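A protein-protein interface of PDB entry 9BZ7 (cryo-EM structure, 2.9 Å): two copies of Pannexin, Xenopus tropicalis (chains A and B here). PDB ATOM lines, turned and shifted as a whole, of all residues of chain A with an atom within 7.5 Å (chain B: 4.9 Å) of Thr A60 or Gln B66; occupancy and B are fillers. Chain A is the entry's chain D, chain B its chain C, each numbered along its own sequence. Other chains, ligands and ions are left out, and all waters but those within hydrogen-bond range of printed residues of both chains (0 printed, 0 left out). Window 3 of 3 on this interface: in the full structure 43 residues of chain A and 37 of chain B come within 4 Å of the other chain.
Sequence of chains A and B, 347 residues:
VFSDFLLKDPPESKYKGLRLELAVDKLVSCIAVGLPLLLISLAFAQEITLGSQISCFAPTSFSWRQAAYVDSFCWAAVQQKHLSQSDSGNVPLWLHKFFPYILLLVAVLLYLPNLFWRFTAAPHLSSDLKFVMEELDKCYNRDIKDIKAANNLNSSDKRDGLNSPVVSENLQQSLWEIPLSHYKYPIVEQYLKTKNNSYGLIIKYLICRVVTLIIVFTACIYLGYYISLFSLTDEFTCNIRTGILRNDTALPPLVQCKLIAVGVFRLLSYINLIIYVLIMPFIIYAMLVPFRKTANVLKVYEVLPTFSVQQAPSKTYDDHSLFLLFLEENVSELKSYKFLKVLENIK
NE2 of Gln B66 lies close to N of Thr A60, 3.5 Å away. O of Ala A58 sits at hydrogen-bond distance from NE2 of Gln B66 (2.5 Å).
N of Ser B63 is in hydrogen-bond range of OE1 of Gln B66 (3.5 Å).
Among the printed residues, pairs that only touch across the chains: Cys A56 with Tyr B69 (3.7 Å), Phe A57 with Gln B66 (3.3 Å), Phe A57 with Tyr B69 (3.4 Å), Pro A59 with Gln B66 (3.6 Å) and Ala A67 with Arg B65 (3.3 Å).
Printed residues of chain B within 4 Å of Cys A56: Tyr B69. Printed residues of chain B within 4 Å of Pro A59: Gln B66. Thr A60 touches just one residue of chain B: Gln B66. Gln A66 touches none of the printed residues of chain B. Printed residues of chain B within 4 Å of Ala A67: Arg B65 (3.3 Å). Trp B64 touches none of the printed residues of chain A.
Of the 10 printed residues of chain B, 3 touch a printed residue of chain A. Printed residues of chain B that touch a printed residue of chain A: Arg B65, Gln B66 and Tyr B69. Along chain A the printed residues that touch a printed residue of chain B span positions 56 to 67. Among the printed residues, no Asp or Glu carboxylate lies within 4 Å of a Lys or Arg side-chain nitrogen of the other chain.
Positions printed for both chains: 61, 62, 63, 66 and 67.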
ATOM      1  N   CYS A  56     -13.199  12.297   1.940  1.00  0.00           N
ATOM      2  CA  CYS A  56     -14.353  13.048   2.412  1.00  0.00           C
ATOM      3  C   CYS A  56     -15.268  12.139   3.220  1.00  0.00           C
ATOM      4  O   CYS A  56     -15.508  10.987   2.841  1.00  0.00           O
ATOM      5  CB  CYS A  56     -15.130  13.671   1.247  1.00  0.00           C
ATOM      6  SG  CYS A  56     -14.149  14.756   0.186  1.00  0.00           S
ATOM      7  N   PHE A  57     -15.776  12.661   4.333  1.00  0.00           N
ATOM      8  CA  PHE A  57     -16.685  11.913   5.196  1.00  0.00           C
ATOM      9  C   PHE A  57     -18.098  12.017   4.637  1.00  0.00           C
ATOM     10  O   PHE A  57     -18.715  13.087   4.680  1.00  0.00           O
ATOM     11  CB  PHE A  57     -16.620  12.440   6.626  1.00  0.00           C
ATOM     12  CG  PHE A  57     -17.377  11.598   7.616  1.00  0.00           C
ATOM     13  CD1 PHE A  57     -16.868  10.386   8.052  1.00  0.00           C
ATOM     14  CD2 PHE A  57     -18.599  12.023   8.114  1.00  0.00           C
ATOM     15  CE1 PHE A  57     -17.562   9.612   8.963  1.00  0.00           C
ATOM     16  CE2 PHE A  57     -19.297  11.252   9.026  1.00  0.00           C
ATOM     17  CZ  PHE A  57     -18.778  10.046   9.450  1.00  0.00           C
ATOM     18  N   ALA A  58     -18.610  10.912   4.116  1.00  0.00           N
ATOM     19  CA  ALA A  58     -19.947  10.844   3.552  1.00  0.00           C
ATOM     20  C   ALA A  58     -20.932  10.292   4.572  1.00  0.00           C
ATOM     21  O   ALA A  58     -20.560   9.514   5.456  1.00  0.00           O
ATOM     22  CB  ALA A  58     -19.950   9.966   2.298  1.00  0.00           C
ATOM     23  N   PRO A  59     -22.201  10.682   4.485  1.00  0.00           N
ATOM     24  CA  PRO A  59     -23.203  10.138   5.408  1.00  0.00           C
ATOM     25  C   PRO A  59     -23.413   8.648   5.191  1.00  0.00           C
ATOM     26  O   PRO A  59     -23.175   8.103   4.109  1.00  0.00           O
ATOM     27  CB  PRO A  59     -24.471  10.932   5.069  1.00  0.00           C
ATOM     28  CG  PRO A  59     -24.243  11.448   3.686  1.00  0.00           C
ATOM     29  CD  PRO A  59     -22.771  11.704   3.591  1.00  0.00           C
ATOM     30  N   THR A  60     -23.863   7.982   6.258  1.00  0.00           N
ATOM     31  CA  THR A  60     -24.073   6.538   6.203  1.00  0.00           C
ATOM     32  C   THR A  60     -25.149   6.161   5.192  1.00  0.00           C
ATOM     33  O   THR A  60     -25.136   5.043   4.664  1.00  0.00           O
ATOM     34  CB  THR A  60     -24.444   6.006   7.587  1.00  0.00           C
ATOM     35  OG1 THR A  60     -25.719   6.530   7.979  1.00  0.00           O
ATOM     36  CG2 THR A  60     -23.397   6.416   8.613  1.00  0.00           C
ATOM     37  N   SER A  61     -26.087   7.070   4.915  1.00  0.00           N
ATOM     38  CA  SER A  61     -27.129   6.782   3.934  1.00  0.00           C
ATOM     39  C   SER A  61     -26.557   6.635   2.531  1.00  0.00           C
ATOM     40  O   SER A  61     -27.127   5.919   1.700  1.00  0.00           O
ATOM     41  CB  SER A  61     -28.192   7.880   3.962  1.00  0.00           C
ATOM     42  OG  SER A  61     -27.603   9.154   4.161  1.00  0.00           O
ATOM     43  N   PHE A  62     -25.440   7.302   2.247  1.00  0.00           N
ATOM     44  CA  PHE A  62     -24.836   7.221   0.923  1.00  0.00           C
ATOM     45  C   PHE A  62     -24.257   5.834   0.678  1.00  0.00           C
ATOM     46  O   PHE A  62     -23.740   5.185   1.593  1.00  0.00           O
ATOM     47  CB  PHE A  62     -23.741   8.278   0.775  1.00  0.00           C
ATOM     48  CG  PHE A  62     -24.254   9.635   0.382  1.00  0.00           C
ATOM     49  CD1 PHE A  62     -25.607   9.923   0.430  1.00  0.00           C
ATOM     50  CD2 PHE A  62     -23.379  10.623  -0.036  1.00  0.00           C
ATOM     51  CE1 PHE A  62     -26.078  11.169   0.069  1.00  0.00           C
ATOM     52  CE2 PHE A  62     -23.844  11.873  -0.398  1.00  0.00           C
ATOM     53  CZ  PHE A  62     -25.197  12.146  -0.345  1.00  0.00           C
ATOM     54  N   SER A  63     -24.345   5.380  -0.569  1.00  0.00           N
ATOM     55  CA  SER A  63     -23.764   4.106  -0.966  1.00  0.00           C
ATOM     56  C   SER A  63     -22.289   4.309  -1.313  1.00  0.00           C
ATOM     57  O   SER A  63     -21.709   5.373  -1.077  1.00  0.00           O
ATOM     58  CB  SER A  63     -24.551   3.502  -2.127  1.00  0.00           C
ATOM     59  OG  SER A  63     -24.942   4.501  -3.053  1.00  0.00           O
ATOM     60  N   GLN A  66     -22.032   6.782  -4.536  1.00  0.00           N
ATOM     61  CA  GLN A  66     -22.344   8.164  -4.183  1.00  0.00           C
ATOM     62  C   GLN A  66     -21.174   8.819  -3.460  1.00  0.00           C
ATOM     63  O   GLN A  66     -20.831   9.978  -3.729  1.00  0.00           O
ATOM     64  CB  GLN A  66     -23.610   8.218  -3.329  1.00  0.00           C
ATOM     65  CG  GLN A  66     -24.833   7.617  -4.006  1.00  0.00           C
ATOM     66  CD  GLN A  66     -26.120   7.924  -3.267  1.00  0.00           C
ATOM     67  OE1 GLN A  66     -26.155   7.940  -2.038  1.00  0.00           O
ATOM     68  NE2 GLN A  66     -27.188   8.170  -4.017  1.00  0.00           N
ATOM     69  N   ALA A  67     -20.539   8.086  -2.539  1.00  0.00           N
ATOM     70  CA  ALA A  67     -19.343   8.597  -1.882  1.00  0.00           C
ATOM     71  C   ALA A  67     -18.207   8.810  -2.875  1.00  0.00           C
ATOM     72  O   ALA A  67     -17.472   9.797  -2.771  1.00  0.00           O
ATOM     73  CB  ALA A  67     -18.909   7.649  -0.765  1.00  0.00           C
ATOM     74  N   SER B  61     -21.199   0.878  12.941  1.00  0.00           N
ATOM     75  CA  SER B  61     -22.139   1.759  12.253  1.00  0.00           C
ATOM     76  C   SER B  61     -21.504   2.421  11.037  1.00  0.00           C
ATOM     77  O   SER B  61     -22.205   2.757  10.077  1.00  0.00           O
ATOM     78  CB  SER B  61     -22.667   2.819  13.219  1.00  0.00           C
ATOM     79  OG  SER B  61     -21.647   3.259  14.099  1.00  0.00           O
ATOM     80  N   PHE B  62     -20.187   2.620  11.060  1.00  0.00           N
ATOM     81  CA  PHE B  62     -19.507   3.257   9.940  1.00  0.00           C
ATOM     82  C   PHE B  62     -19.506   2.345   8.721  1.00  0.00           C
ATOM     83  O   PHE B  62     -19.410   1.121   8.838  1.00  0.00           O
ATOM     84  CB  PHE B  62     -18.071   3.614  10.326  1.00  0.00           C
ATOM     85  CG  PHE B  62     -17.944   4.921  11.057  1.00  0.00           C
ATOM     86  CD1 PHE B  62     -19.064   5.567  11.553  1.00  0.00           C
ATOM     87  CD2 PHE B  62     -16.702   5.503  11.249  1.00  0.00           C
ATOM     88  CE1 PHE B  62     -18.948   6.769  12.224  1.00  0.00           C
ATOM     89  CE2 PHE B  62     -16.579   6.703  11.920  1.00  0.00           C
ATOM     90  CZ  PHE B  62     -17.703   7.337  12.407  1.00  0.00           C
ATOM     91  N   SER B  63     -19.612   2.952   7.542  1.00  0.00           N
ATOM     92  CA  SER B  63     -19.546   2.216   6.288  1.00  0.00           C
ATOM     93  C   SER B  63     -18.083   2.035   5.885  1.00  0.00           C
ATOM     94  O   SER B  63     -17.160   2.323   6.653  1.00  0.00           O
ATOM     95  CB  SER B  63     -20.360   2.929   5.211  1.00  0.00           C
ATOM     96  OG  SER B  63     -20.199   4.334   5.295  1.00  0.00           O
ATOM     97  N   TRP B  64     -17.855   1.546   4.665  1.00  0.00           N
ATOM     98  CA  TRP B  64     -16.490   1.330   4.194  1.00  0.00           C
ATOM     99  C   TRP B  64     -15.755   2.653   4.020  1.00  0.00           C
ATOM    100  O   TRP B  64     -14.635   2.827   4.519  1.00  0.00           O
ATOM    101  CB  TRP B  64     -16.512   0.553   2.878  1.00  0.00           C
ATOM    102  CG  TRP B  64     -15.162   0.084   2.407  1.00  0.00           C
ATOM    103  CD1 TRP B  64     -14.083   0.859   2.086  1.00  0.00           C
ATOM    104  CD2 TRP B  64     -14.763  -1.272   2.173  1.00  0.00           C
ATOM    105  NE1 TRP B  64     -13.034   0.069   1.684  1.00  0.00           N
ATOM    106  CE2 TRP B  64     -13.426  -1.243   1.726  1.00  0.00           C
ATOM    107  CE3 TRP B  64     -15.405  -2.506   2.300  1.00  0.00           C
ATOM    108  CZ2 TRP B  64     -12.720  -2.402   1.411  1.00  0.00           C
ATOM    109  CZ3 TRP B  64     -14.704  -3.654   1.986  1.00  0.00           C
ATOM    110  CH2 TRP B  64     -13.376  -3.594   1.548  1.00  0.00           C
ATOM    111  N   ARG B  65     -16.370   3.600   3.314  1.00  0.00           N
ATOM    112  CA  ARG B  65     -15.719   4.862   2.998  1.00  0.00           C
ATOM    113  C   ARG B  65     -15.562   5.777   4.203  1.00  0.00           C
ATOM    114  O   ARG B  65     -14.604   6.552   4.244  1.00  0.00           O
ATOM    115  CB  ARG B  65     -16.480   5.594   1.885  1.00  0.00           C
ATOM    116  CG  ARG B  65     -17.060   4.661   0.834  1.00  0.00           C
ATOM    117  CD  ARG B  65     -15.973   4.177  -0.116  1.00  0.00           C
ATOM    118  NE  ARG B  65     -15.090   5.254  -0.548  1.00  0.00           N
ATOM    119  CZ  ARG B  65     -15.357   6.091  -1.540  1.00  0.00           C
ATOM    120  NH1 ARG B  65     -16.471   5.993  -2.246  1.00  0.00           N
ATOM    121  NH2 ARG B  65     -14.478   7.045  -1.838  1.00  0.00           N
ATOM    122  N   GLN B  66     -16.459   5.702   5.189  1.00  0.00           N
ATOM    123  CA  GLN B  66     -16.232   6.438   6.430  1.00  0.00           C
ATOM    124  C   GLN B  66     -14.996   5.915   7.155  1.00  0.00           C
ATOM    125  O   GLN B  66     -14.189   6.697   7.670  1.00  0.00           O
ATOM    126  CB  GLN B  66     -17.467   6.352   7.326  1.00  0.00           C
ATOM    127  CG  GLN B  66     -18.733   6.895   6.682  1.00  0.00           C
ATOM    128  CD  GLN B  66     -19.870   7.054   7.672  1.00  0.00           C
ATOM    129  OE1 GLN B  66     -20.048   6.231   8.567  1.00  0.00           O
ATOM    130  NE2 GLN B  66     -20.647   8.119   7.510  1.00  0.00           N
ATOM    131  N   ALA B  67     -14.829   4.590   7.194  1.00  0.00           N
ATOM    132  CA  ALA B  67     -13.620   4.015   7.770  1.00  0.00           C
ATOM    133  C   ALA B  67     -12.380   4.410   6.978  1.00  0.00           C
ATOM    134  O   ALA B  67     -11.331   4.683   7.568  1.00  0.00           O
ATOM    135  CB  ALA B  67     -13.745   2.493   7.846  1.00  0.00           C
ATOM    136  N   ALA B  68     -12.481   4.449   5.648  1.00  0.00           N
ATOM    137  CA  ALA B  68     -11.354   4.909   4.842  1.00  0.00           C
ATOM    138  C   ALA B  68     -11.018   6.366   5.144  1.00  0.00           C
ATOM    139  O   ALA B  68      -9.841   6.738   5.217  1.00  0.00           O
ATOM    140  CB  ALA B  68     -11.659   4.724   3.356  1.00  0.00           C
ATOM    141  N   TYR B  69     -12.042   7.203   5.320  1.00  0.00           N
ATOM    142  CA  TYR B  69     -11.813   8.608   5.640  1.00  0.00           C
ATOM    143  C   TYR B  69     -11.131   8.765   6.991  1.00  0.00           C
ATOM    144  O   TYR B  69     -10.209   9.575   7.134  1.00  0.00           O
ATOM    145  CB  TYR B  69     -13.133   9.379   5.620  1.00  0.00           C
ATOM    146  CG  TYR B  69     -13.046  10.735   6.285  1.00  0.00           C
ATOM    147  CD1 TYR B  69     -12.470  11.815   5.628  1.00  0.00           C
ATOM    148  CD2 TYR B  69     -13.531  10.934   7.571  1.00  0.00           C
ATOM    149  CE1 TYR B  69     -12.384  13.055   6.233  1.00  0.00           C
ATOM    150  CE2 TYR B  69     -13.449  12.169   8.184  1.00  0.00           C
ATOM    151  CZ  TYR B  69     -12.876  13.226   7.511  1.00  0.00           C
ATOM    152  OH  TYR B  69     -12.793  14.459   8.117  1.00  0.00           O
ATOM    153  N   VAL B  70     -11.579   8.015   8.002  1.00  0.00           N
ATOM    154  CA  VAL B  70     -10.924   8.127   9.305  1.00  0.00           C
ATOM    155  C   VAL B  70      -9.503   7.572   9.242  1.00  0.00           C
ATOM    156  O   VAL B  70      -8.598   8.102   9.899  1.00  0.00           O
ATOM    157  CB  VAL B  70     -11.759   7.467  10.423  1.00  0.00           C
ATOM    158  CG1 VAL B  70     -13.208   7.928  10.351  1.00  0.00           C
ATOM    159  CG2 VAL B  70     -11.672   5.950  10.375  1.00  0.00           C
